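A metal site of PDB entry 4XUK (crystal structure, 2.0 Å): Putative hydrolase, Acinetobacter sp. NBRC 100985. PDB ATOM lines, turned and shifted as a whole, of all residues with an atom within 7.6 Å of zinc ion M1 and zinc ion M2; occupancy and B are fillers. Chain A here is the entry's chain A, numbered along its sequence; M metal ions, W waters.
O of Ser 57 sits at hydrogen-bond distance from ND1 of His 265, 2.9 Å away. ND1 of His 197 sits at hydrogen-bond distance from OD1 of Asp 237 (2.8 Å). ND1 of His 113 lies within hydrogen-bond range of OD2 of Asp 73, 2.8 Å away. The side-chain hydroxyl (OG1) of Thr 107 lies within hydrogen-bond range of a ring nitrogen (ND1) of His 108 (2.8 Å). The backbone NH (N) of Asp 218 is in hydrogen-bond range of a ring nitrogen (NE2) of His 201, at 2.8 Å.
Four residues have an atom within 4 Å of zinc ion M1: Asp 112, His 113, Asp 218 and His 265.
Within 4 Å of zinc ion M2: His 108, His 110, His 113, His 197 and Asp 218.
Zinc ion M1 is bound by NE2 of His 113 (2.0 Å). Zinc ion M1 is bound by OD2 of Asp 218 (2.1 Å). Zinc ion M1 is bound by NE2 of His 265, 2.2 Å away. OD2 of Asp 112 binds zinc ion M1, 2.3 Å away. Zinc ion M1 has four donor atoms within binding distance.
Zinc ion M2 is bound by NE2 of His 197, at 2.2 Å. NE2 of His 108 is bound to zinc ion M2, 2.3 Å away. Zinc ion M2 is bound by ND1 of His 110. Zinc ion M2 is bound by the side-chain carboxylate (OD2) of Asp 218.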
ATOM      1  N   SER A  57      21.482  -6.477  -1.655  1.00  0.00           N
ATOM      2  CA  SER A  57      20.518  -5.549  -2.223  1.00  0.00           C
ATOM      3  C   SER A  57      19.655  -6.246  -3.273  1.00  0.00           C
ATOM      4  O   SER A  57      20.050  -7.257  -3.868  1.00  0.00           O
ATOM      5  CB  SER A  57      21.236  -4.358  -2.862  1.00  0.00           C
ATOM      6  OG  SER A  57      21.972  -3.614  -1.918  1.00  0.00           O
ATOM      7  N   ILE A  58      18.463  -5.690  -3.485  1.00  0.00           N
ATOM      8  CA  ILE A  58      17.645  -6.052  -4.620  1.00  0.00           C
ATOM      9  C   ILE A  58      17.364  -4.736  -5.324  1.00  0.00           C
ATOM     10  O   ILE A  58      16.714  -3.855  -4.770  1.00  0.00           O
ATOM     11  CB  ILE A  58      16.312  -6.720  -4.199  1.00  0.00           C
ATOM     12  CG1 ILE A  58      16.548  -7.996  -3.391  1.00  0.00           C
ATOM     13  CG2 ILE A  58      15.482  -7.077  -5.451  1.00  0.00           C
ATOM     14  CD1 ILE A  58      16.755  -7.752  -1.898  1.00  0.00           C
ATOM     15  N   ASN A  59      17.893  -4.589  -6.535  1.00  0.00           N
ATOM     16  CA  ASN A  59      17.764  -3.350  -7.286  1.00  0.00           C
ATOM     17  C   ASN A  59      16.995  -3.549  -8.607  1.00  0.00           C
ATOM     18  O   ASN A  59      16.852  -4.688  -9.107  1.00  0.00           O
ATOM     19  CB  ASN A  59      19.137  -2.761  -7.610  1.00  0.00           C
ATOM     20  CG  ASN A  59      20.086  -2.759  -6.422  1.00  0.00           C
ATOM     21  OD1 ASN A  59      19.749  -2.300  -5.333  1.00  0.00           O
ATOM     22  ND2 ASN A  59      21.290  -3.252  -6.641  1.00  0.00           N
ATOM     23  N   ASP A  73      14.040  -5.054 -14.927  1.00  0.00           N
ATOM     24  CA  ASP A  73      13.550  -5.663 -13.684  1.00  0.00           C
ATOM     25  C   ASP A  73      12.731  -4.667 -12.843  1.00  0.00           C
ATOM     26  O   ASP A  73      12.723  -3.473 -13.135  1.00  0.00           O
ATOM     27  CB  ASP A  73      14.686  -6.353 -12.888  1.00  0.00           C
ATOM     28  CG  ASP A  73      15.240  -7.555 -13.621  1.00  0.00           C
ATOM     29  OD1 ASP A  73      14.536  -8.057 -14.538  1.00  0.00           O
ATOM     30  OD2 ASP A  73      16.376  -7.992 -13.313  1.00  0.00           O
ATOM     31  N   PHE A  80       7.399 -11.332  -1.707  1.00  0.00           N
ATOM     32  CA  PHE A  80       8.378 -11.899  -0.761  1.00  0.00           C
ATOM     33  C   PHE A  80       8.290 -11.249   0.592  1.00  0.00           C
ATOM     34  O   PHE A  80       9.244 -11.286   1.379  1.00  0.00           O
ATOM     35  CB  PHE A  80       9.813 -11.747  -1.294  1.00  0.00           C
ATOM     36  CG  PHE A  80      10.220 -12.831  -2.256  1.00  0.00           C
ATOM     37  CD1 PHE A  80       9.695 -14.112  -2.145  1.00  0.00           C
ATOM     38  CD2 PHE A  80      11.137 -12.564  -3.265  1.00  0.00           C
ATOM     39  CE1 PHE A  80      10.082 -15.108  -3.031  1.00  0.00           C
ATOM     40  CE2 PHE A  80      11.531 -13.564  -4.144  1.00  0.00           C
ATOM     41  CZ  PHE A  80      10.993 -14.833  -4.030  1.00  0.00           C
ATOM     42  N   THR A 107      15.149  -9.736 -16.792  1.00  0.00           N
ATOM     43  CA  THR A 107      16.296 -10.626 -16.960  1.00  0.00           C
ATOM     44  C   THR A 107      15.859 -12.075 -16.809  1.00  0.00           C
ATOM     45  O   THR A 107      16.381 -12.962 -17.507  1.00  0.00           O
ATOM     46  CB  THR A 107      17.423 -10.313 -15.964  1.00  0.00           C
ATOM     47  OG1 THR A 107      16.911 -10.365 -14.621  1.00  0.00           O
ATOM     48  CG2 THR A 107      18.006  -8.935 -16.257  1.00  0.00           C
ATOM     49  N   HIS A 108      14.896 -12.295 -15.923  1.00  0.00           N
ATOM     50  CA  HIS A 108      14.290 -13.608 -15.694  1.00  0.00           C
ATOM     51  C   HIS A 108      13.023 -13.433 -14.871  1.00  0.00           C
ATOM     52  O   HIS A 108      12.709 -12.316 -14.432  1.00  0.00           O
ATOM     53  CB  HIS A 108      15.255 -14.596 -14.996  1.00  0.00           C
ATOM     54  CG  HIS A 108      15.792 -14.107 -13.682  1.00  0.00           C
ATOM     55  ND1 HIS A 108      16.331 -12.849 -13.511  1.00  0.00           N
ATOM     56  CD2 HIS A 108      15.903 -14.741 -12.492  1.00  0.00           C
ATOM     57  CE1 HIS A 108      16.734 -12.720 -12.258  1.00  0.00           C
ATOM     58  NE2 HIS A 108      16.490 -13.850 -11.627  1.00  0.00           N
ATOM     59  N   LEU A 109      12.302 -14.525 -14.631  1.00  0.00           N
ATOM     60  CA  LEU A 109      10.985 -14.430 -14.003  1.00  0.00           C
ATOM     61  C   LEU A 109      10.958 -14.790 -12.508  1.00  0.00           C
ATOM     62  O   LEU A 109       9.887 -15.035 -11.969  1.00  0.00           O
ATOM     63  CB  LEU A 109       9.971 -15.290 -14.772  1.00  0.00           C
ATOM     64  CG  LEU A 109       9.667 -14.853 -16.209  1.00  0.00           C
ATOM     65  CD1 LEU A 109       8.777 -15.882 -16.914  1.00  0.00           C
ATOM     66  CD2 LEU A 109       8.978 -13.510 -16.211  1.00  0.00           C
ATOM     67  N   HIS A 110      12.114 -14.798 -11.839  1.00  0.00           N
ATOM     68  CA  HIS A 110      12.104 -14.928 -10.380  1.00  0.00           C
ATOM     69  C   HIS A 110      11.272 -13.758  -9.822  1.00  0.00           C
ATOM     70  O   HIS A 110      11.293 -12.662 -10.376  1.00  0.00           O
ATOM     71  CB  HIS A 110      13.542 -14.976  -9.791  1.00  0.00           C
ATOM     72  CG  HIS A 110      14.089 -16.372  -9.697  1.00  0.00           C
ATOM     73  ND1 HIS A 110      15.427 -16.633  -9.537  1.00  0.00           N
ATOM     74  CD2 HIS A 110      13.471 -17.583  -9.727  1.00  0.00           C
ATOM     75  CE1 HIS A 110      15.625 -17.937  -9.493  1.00  0.00           C
ATOM     76  NE2 HIS A 110      14.450 -18.538  -9.608  1.00  0.00           N
ATOM     77  N   PRO A 111      10.509 -14.011  -8.747  1.00  0.00           N
ATOM     78  CA  PRO A 111       9.574 -13.001  -8.228  1.00  0.00           C
ATOM     79  C   PRO A 111      10.204 -11.666  -7.843  1.00  0.00           C
ATOM     80  O   PRO A 111       9.517 -10.653  -7.918  1.00  0.00           O
ATOM     81  CB  PRO A 111       8.997 -13.690  -6.984  1.00  0.00           C
ATOM     82  CG  PRO A 111       9.038 -15.168  -7.355  1.00  0.00           C
ATOM     83  CD  PRO A 111      10.352 -15.318  -8.079  1.00  0.00           C
ATOM     84  N   ASP A 112      11.483 -11.655  -7.455  1.00  0.00           N
ATOM     85  CA  ASP A 112      12.098 -10.394  -7.064  1.00  0.00           C
ATOM     86  C   ASP A 112      12.537  -9.568  -8.285  1.00  0.00           C
ATOM     87  O   ASP A 112      13.183  -8.533  -8.148  1.00  0.00           O
ATOM     88  CB  ASP A 112      13.268 -10.641  -6.101  1.00  0.00           C
ATOM     89  CG  ASP A 112      14.271 -11.634  -6.648  1.00  0.00           C
ATOM     90  OD1 ASP A 112      13.852 -12.676  -7.190  1.00  0.00           O
ATOM     91  OD2 ASP A 112      15.474 -11.368  -6.531  1.00  0.00           O
ATOM     92  N   HIS A 113      12.154 -10.030  -9.470  1.00  0.00           N
ATOM     93  CA  HIS A 113      12.412  -9.278 -10.688  1.00  0.00           C
ATOM     94  C   HIS A 113      11.146  -8.955 -11.452  1.00  0.00           C
ATOM     95  O   HIS A 113      11.043  -7.863 -12.052  1.00  0.00           O
ATOM     96  CB  HIS A 113      13.404 -10.055 -11.557  1.00  0.00           C
ATOM     97  CG  HIS A 113      14.685 -10.343 -10.849  1.00  0.00           C
ATOM     98  ND1 HIS A 113      15.830  -9.624 -11.070  1.00  0.00           N
ATOM     99  CD2 HIS A 113      14.970 -11.208  -9.846  1.00  0.00           C
ATOM    100  CE1 HIS A 113      16.778 -10.058 -10.265  1.00  0.00           C
ATOM    101  NE2 HIS A 113      16.290 -11.029  -9.517  1.00  0.00           N
ATOM    102  N   GLU A 136      12.790 -18.449 -21.160  1.00  0.00           N
ATOM    103  CA  GLU A 136      12.423 -18.195 -19.763  1.00  0.00           C
ATOM    104  C   GLU A 136      10.932 -18.399 -19.550  1.00  0.00           C
ATOM    105  O   GLU A 136      10.520 -19.073 -18.601  1.00  0.00           O
ATOM    106  CB  GLU A 136      12.843 -16.789 -19.336  1.00  0.00           C
ATOM    107  CG  GLU A 136      12.538 -16.469 -17.879  1.00  0.00           C
ATOM    108  CD  GLU A 136      13.469 -17.166 -16.893  1.00  0.00           C
ATOM    109  OE1 GLU A 136      14.446 -17.805 -17.332  1.00  0.00           O
ATOM    110  OE2 GLU A 136      13.237 -17.044 -15.672  1.00  0.00           O
ATOM    111  N   HIS A 197      21.370 -19.593 -14.054  1.00  0.00           N
ATOM    112  CA  HIS A 197      20.591 -19.178 -12.891  1.00  0.00           C
ATOM    113  C   HIS A 197      19.127 -19.567 -13.069  1.00  0.00           C
ATOM    114  O   HIS A 197      18.491 -20.064 -12.144  1.00  0.00           O
ATOM    115  CB  HIS A 197      20.708 -17.680 -12.688  1.00  0.00           C
ATOM    116  CG  HIS A 197      19.919 -17.168 -11.527  1.00  0.00           C
ATOM    117  ND1 HIS A 197      20.194 -17.508 -10.219  1.00  0.00           N
ATOM    118  CD2 HIS A 197      18.866 -16.322 -11.484  1.00  0.00           C
ATOM    119  CE1 HIS A 197      19.337 -16.893  -9.425  1.00  0.00           C
ATOM    120  NE2 HIS A 197      18.525 -16.163 -10.172  1.00  0.00           N
ATOM    121  N   THR A 198      18.593 -19.327 -14.270  1.00  0.00           N
ATOM    122  CA  THR A 198      17.313 -19.900 -14.694  1.00  0.00           C
ATOM    123  C   THR A 198      17.509 -20.332 -16.132  1.00  0.00           C
ATOM    124  O   THR A 198      18.426 -19.852 -16.792  1.00  0.00           O
ATOM    125  CB  THR A 198      16.150 -18.877 -14.637  1.00  0.00           C
ATOM    126  OG1 THR A 198      16.357 -17.851 -15.603  1.00  0.00           O
ATOM    127  CG2 THR A 198      16.003 -18.273 -13.235  1.00  0.00           C
ATOM    128  N   HIS A 201      17.567 -17.178 -18.466  1.00  0.00           N
ATOM    129  CA  HIS A 201      18.119 -15.935 -17.937  1.00  0.00           C
ATOM    130  C   HIS A 201      18.882 -15.210 -19.031  1.00  0.00           C
ATOM    131  O   HIS A 201      19.718 -15.812 -19.713  1.00  0.00           O
ATOM    132  CB  HIS A 201      19.037 -16.203 -16.747  1.00  0.00           C
ATOM    133  CG  HIS A 201      19.470 -14.965 -16.021  1.00  0.00           C
ATOM    134  ND1 HIS A 201      20.490 -14.166 -16.465  1.00  0.00           N
ATOM    135  CD2 HIS A 201      19.004 -14.390 -14.886  1.00  0.00           C
ATOM    136  CE1 HIS A 201      20.647 -13.152 -15.631  1.00  0.00           C
ATOM    137  NE2 HIS A 201      19.741 -13.257 -14.671  1.00  0.00           N
ATOM    138  N   GLY A 217      21.661  -8.842 -14.615  1.00  0.00           N
ATOM    139  CA  GLY A 217      20.730  -9.725 -13.947  1.00  0.00           C
ATOM    140  C   GLY A 217      21.435 -10.537 -12.862  1.00  0.00           C
ATOM    141  O   GLY A 217      22.383 -10.059 -12.230  1.00  0.00           O
ATOM    142  N   ASP A 218      20.976 -11.764 -12.657  1.00  0.00           N
ATOM    143  CA  ASP A 218      21.422 -12.570 -11.530  1.00  0.00           C
ATOM    144  C   ASP A 218      22.520 -13.575 -11.852  1.00  0.00           C
ATOM    145  O   ASP A 218      22.463 -14.724 -11.419  1.00  0.00           O
ATOM    146  CB  ASP A 218      20.229 -13.319 -10.930  1.00  0.00           C
ATOM    147  CG  ASP A 218      19.353 -12.429 -10.087  1.00  0.00           C
ATOM    148  OD1 ASP A 218      19.482 -11.185 -10.177  1.00  0.00           O
ATOM    149  OD2 ASP A 218      18.573 -12.975  -9.296  1.00  0.00           O
ATOM    150  N   ILE A 219      23.537 -13.145 -12.586  1.00  0.00           N
ATOM    151  CA  ILE A 219      24.709 -13.984 -12.796  1.00  0.00           C
ATOM    152  C   ILE A 219      25.622 -13.867 -11.577  1.00  0.00           C
ATOM    153  O   ILE A 219      26.687 -14.499 -11.529  1.00  0.00           O
ATOM    154  CB  ILE A 219      25.476 -13.583 -14.050  1.00  0.00           C
ATOM    155  CG1 ILE A 219      25.987 -12.137 -13.923  1.00  0.00           C
ATOM    156  CG2 ILE A 219      24.574 -13.718 -15.288  1.00  0.00           C
ATOM    157  CD1 ILE A 219      26.873 -11.706 -15.071  1.00  0.00           C
ATOM    158  N   VAL A 220      25.210 -13.063 -10.601  1.00  0.00           N
ATOM    159  CA  VAL A 220      25.957 -12.948  -9.342  1.00  0.00           C
ATOM    160  C   VAL A 220      25.082 -12.399  -8.214  1.00  0.00           C
ATOM    161  O   VAL A 220      24.161 -11.600  -8.447  1.00  0.00           O
ATOM    162  CB  VAL A 220      27.256 -12.104  -9.546  1.00  0.00           C
ATOM    163  CG1 VAL A 220      26.959 -10.599  -9.562  1.00  0.00           C
ATOM    164  CG2 VAL A 220      28.264 -12.434  -8.456  1.00  0.00           C
ATOM    165  N   HIS A 221      25.352 -12.843  -6.980  1.00  0.00           N
ATOM    166  CA  HIS A 221      24.529 -12.471  -5.825  1.00  0.00           C
ATOM    167  C   HIS A 221      25.292 -11.800  -4.693  1.00  0.00           C
ATOM    168  O   HIS A 221      24.745 -11.608  -3.608  1.00  0.00           O
ATOM    169  CB  HIS A 221      23.807 -13.695  -5.284  1.00  0.00           C
ATOM    170  CG  HIS A 221      22.652 -14.138  -6.113  1.00  0.00           C
ATOM    171  ND1 HIS A 221      22.802 -14.644  -7.383  1.00  0.00           N
ATOM    172  CD2 HIS A 221      21.315 -14.104  -5.873  1.00  0.00           C
ATOM    173  CE1 HIS A 221      21.616 -14.925  -7.887  1.00  0.00           C
ATOM    174  NE2 HIS A 221      20.700 -14.606  -6.989  1.00  0.00           N
ATOM    175  N   TYR A 236      20.217 -20.517  -5.102  1.00  0.00           N
ATOM    176  CA  TYR A 236      19.170 -19.963  -5.961  1.00  0.00           C
ATOM    177  C   TYR A 236      19.292 -20.371  -7.434  1.00  0.00           C
ATOM    178  O   TYR A 236      18.302 -20.297  -8.183  1.00  0.00           O
ATOM    179  CB  TYR A 236      19.154 -18.416  -5.871  1.00  0.00           C
ATOM    180  CG  TYR A 236      18.942 -17.848  -4.484  1.00  0.00           C
ATOM    181  CD1 TYR A 236      18.016 -18.394  -3.600  1.00  0.00           C
ATOM    182  CD2 TYR A 236      19.677 -16.750  -4.050  1.00  0.00           C
ATOM    183  CE1 TYR A 236      17.834 -17.870  -2.334  1.00  0.00           C
ATOM    184  CE2 TYR A 236      19.496 -16.216  -2.781  1.00  0.00           C
ATOM    185  CZ  TYR A 236      18.573 -16.782  -1.939  1.00  0.00           C
ATOM    186  OH  TYR A 236      18.385 -16.254  -0.680  1.00  0.00           O
ATOM    187  N   ASP A 237      20.493 -20.749  -7.856  1.00  0.00           N
ATOM    188  CA  ASP A 237      20.720 -21.162  -9.241  1.00  0.00           C
ATOM    189  C   ASP A 237      19.939 -22.453  -9.535  1.00  0.00           C
ATOM    190  O   ASP A 237      20.008 -23.409  -8.765  1.00  0.00           O
ATOM    191  CB  ASP A 237      22.210 -21.412  -9.496  1.00  0.00           C
ATOM    192  CG  ASP A 237      23.040 -20.145  -9.434  1.00  0.00           C
ATOM    193  OD1 ASP A 237      22.487 -19.044  -9.636  1.00  0.00           O
ATOM    194  OD2 ASP A 237      24.264 -20.243  -9.177  1.00  0.00           O
ATOM    195  N   PRO A 264      21.223  -6.299 -10.265  1.00  0.00           N
ATOM    196  CA  PRO A 264      20.158  -6.256  -9.273  1.00  0.00           C
ATOM    197  C   PRO A 264      20.604  -6.709  -7.875  1.00  0.00           C
ATOM    198  O   PRO A 264      19.974  -6.286  -6.905  1.00  0.00           O
ATOM    199  CB  PRO A 264      19.105  -7.223  -9.839  1.00  0.00           C
ATOM    200  CG  PRO A 264      19.861  -8.140 -10.728  1.00  0.00           C
ATOM    201  CD  PRO A 264      20.947  -7.274 -11.331  1.00  0.00           C
ATOM    202  N   HIS A 265      21.652  -7.535  -7.773  1.00  0.00           N
ATOM    203  CA  HIS A 265      22.080  -8.012  -6.456  1.00  0.00           C
ATOM    204  C   HIS A 265      23.481  -7.593  -5.986  1.00  0.00           C
ATOM    205  O   HIS A 265      24.071  -8.275  -5.153  1.00  0.00           O
ATOM    206  CB  HIS A 265      21.961  -9.541  -6.381  1.00  0.00           C
ATOM    207  CG  HIS A 265      20.548 -10.026  -6.450  1.00  0.00           C
ATOM    208  ND1 HIS A 265      19.523  -9.395  -5.781  1.00  0.00           N
ATOM    209  CD2 HIS A 265      19.987 -11.069  -7.107  1.00  0.00           C
ATOM    210  CE1 HIS A 265      18.388 -10.025  -6.035  1.00  0.00           C
ATOM    211  NE2 HIS A 265      18.647 -11.046  -6.826  1.00  0.00           N
HETATM  212 ZN    ZN M   1      17.104 -12.102  -8.020  1.00  0.00          ZN
HETATM  213 ZN    ZN M   2      16.970 -14.783  -9.575  1.00  0.00          ZN
HETATM  214  O   HOH W   1      17.787 -15.115  -6.766  1.00  0.00           O
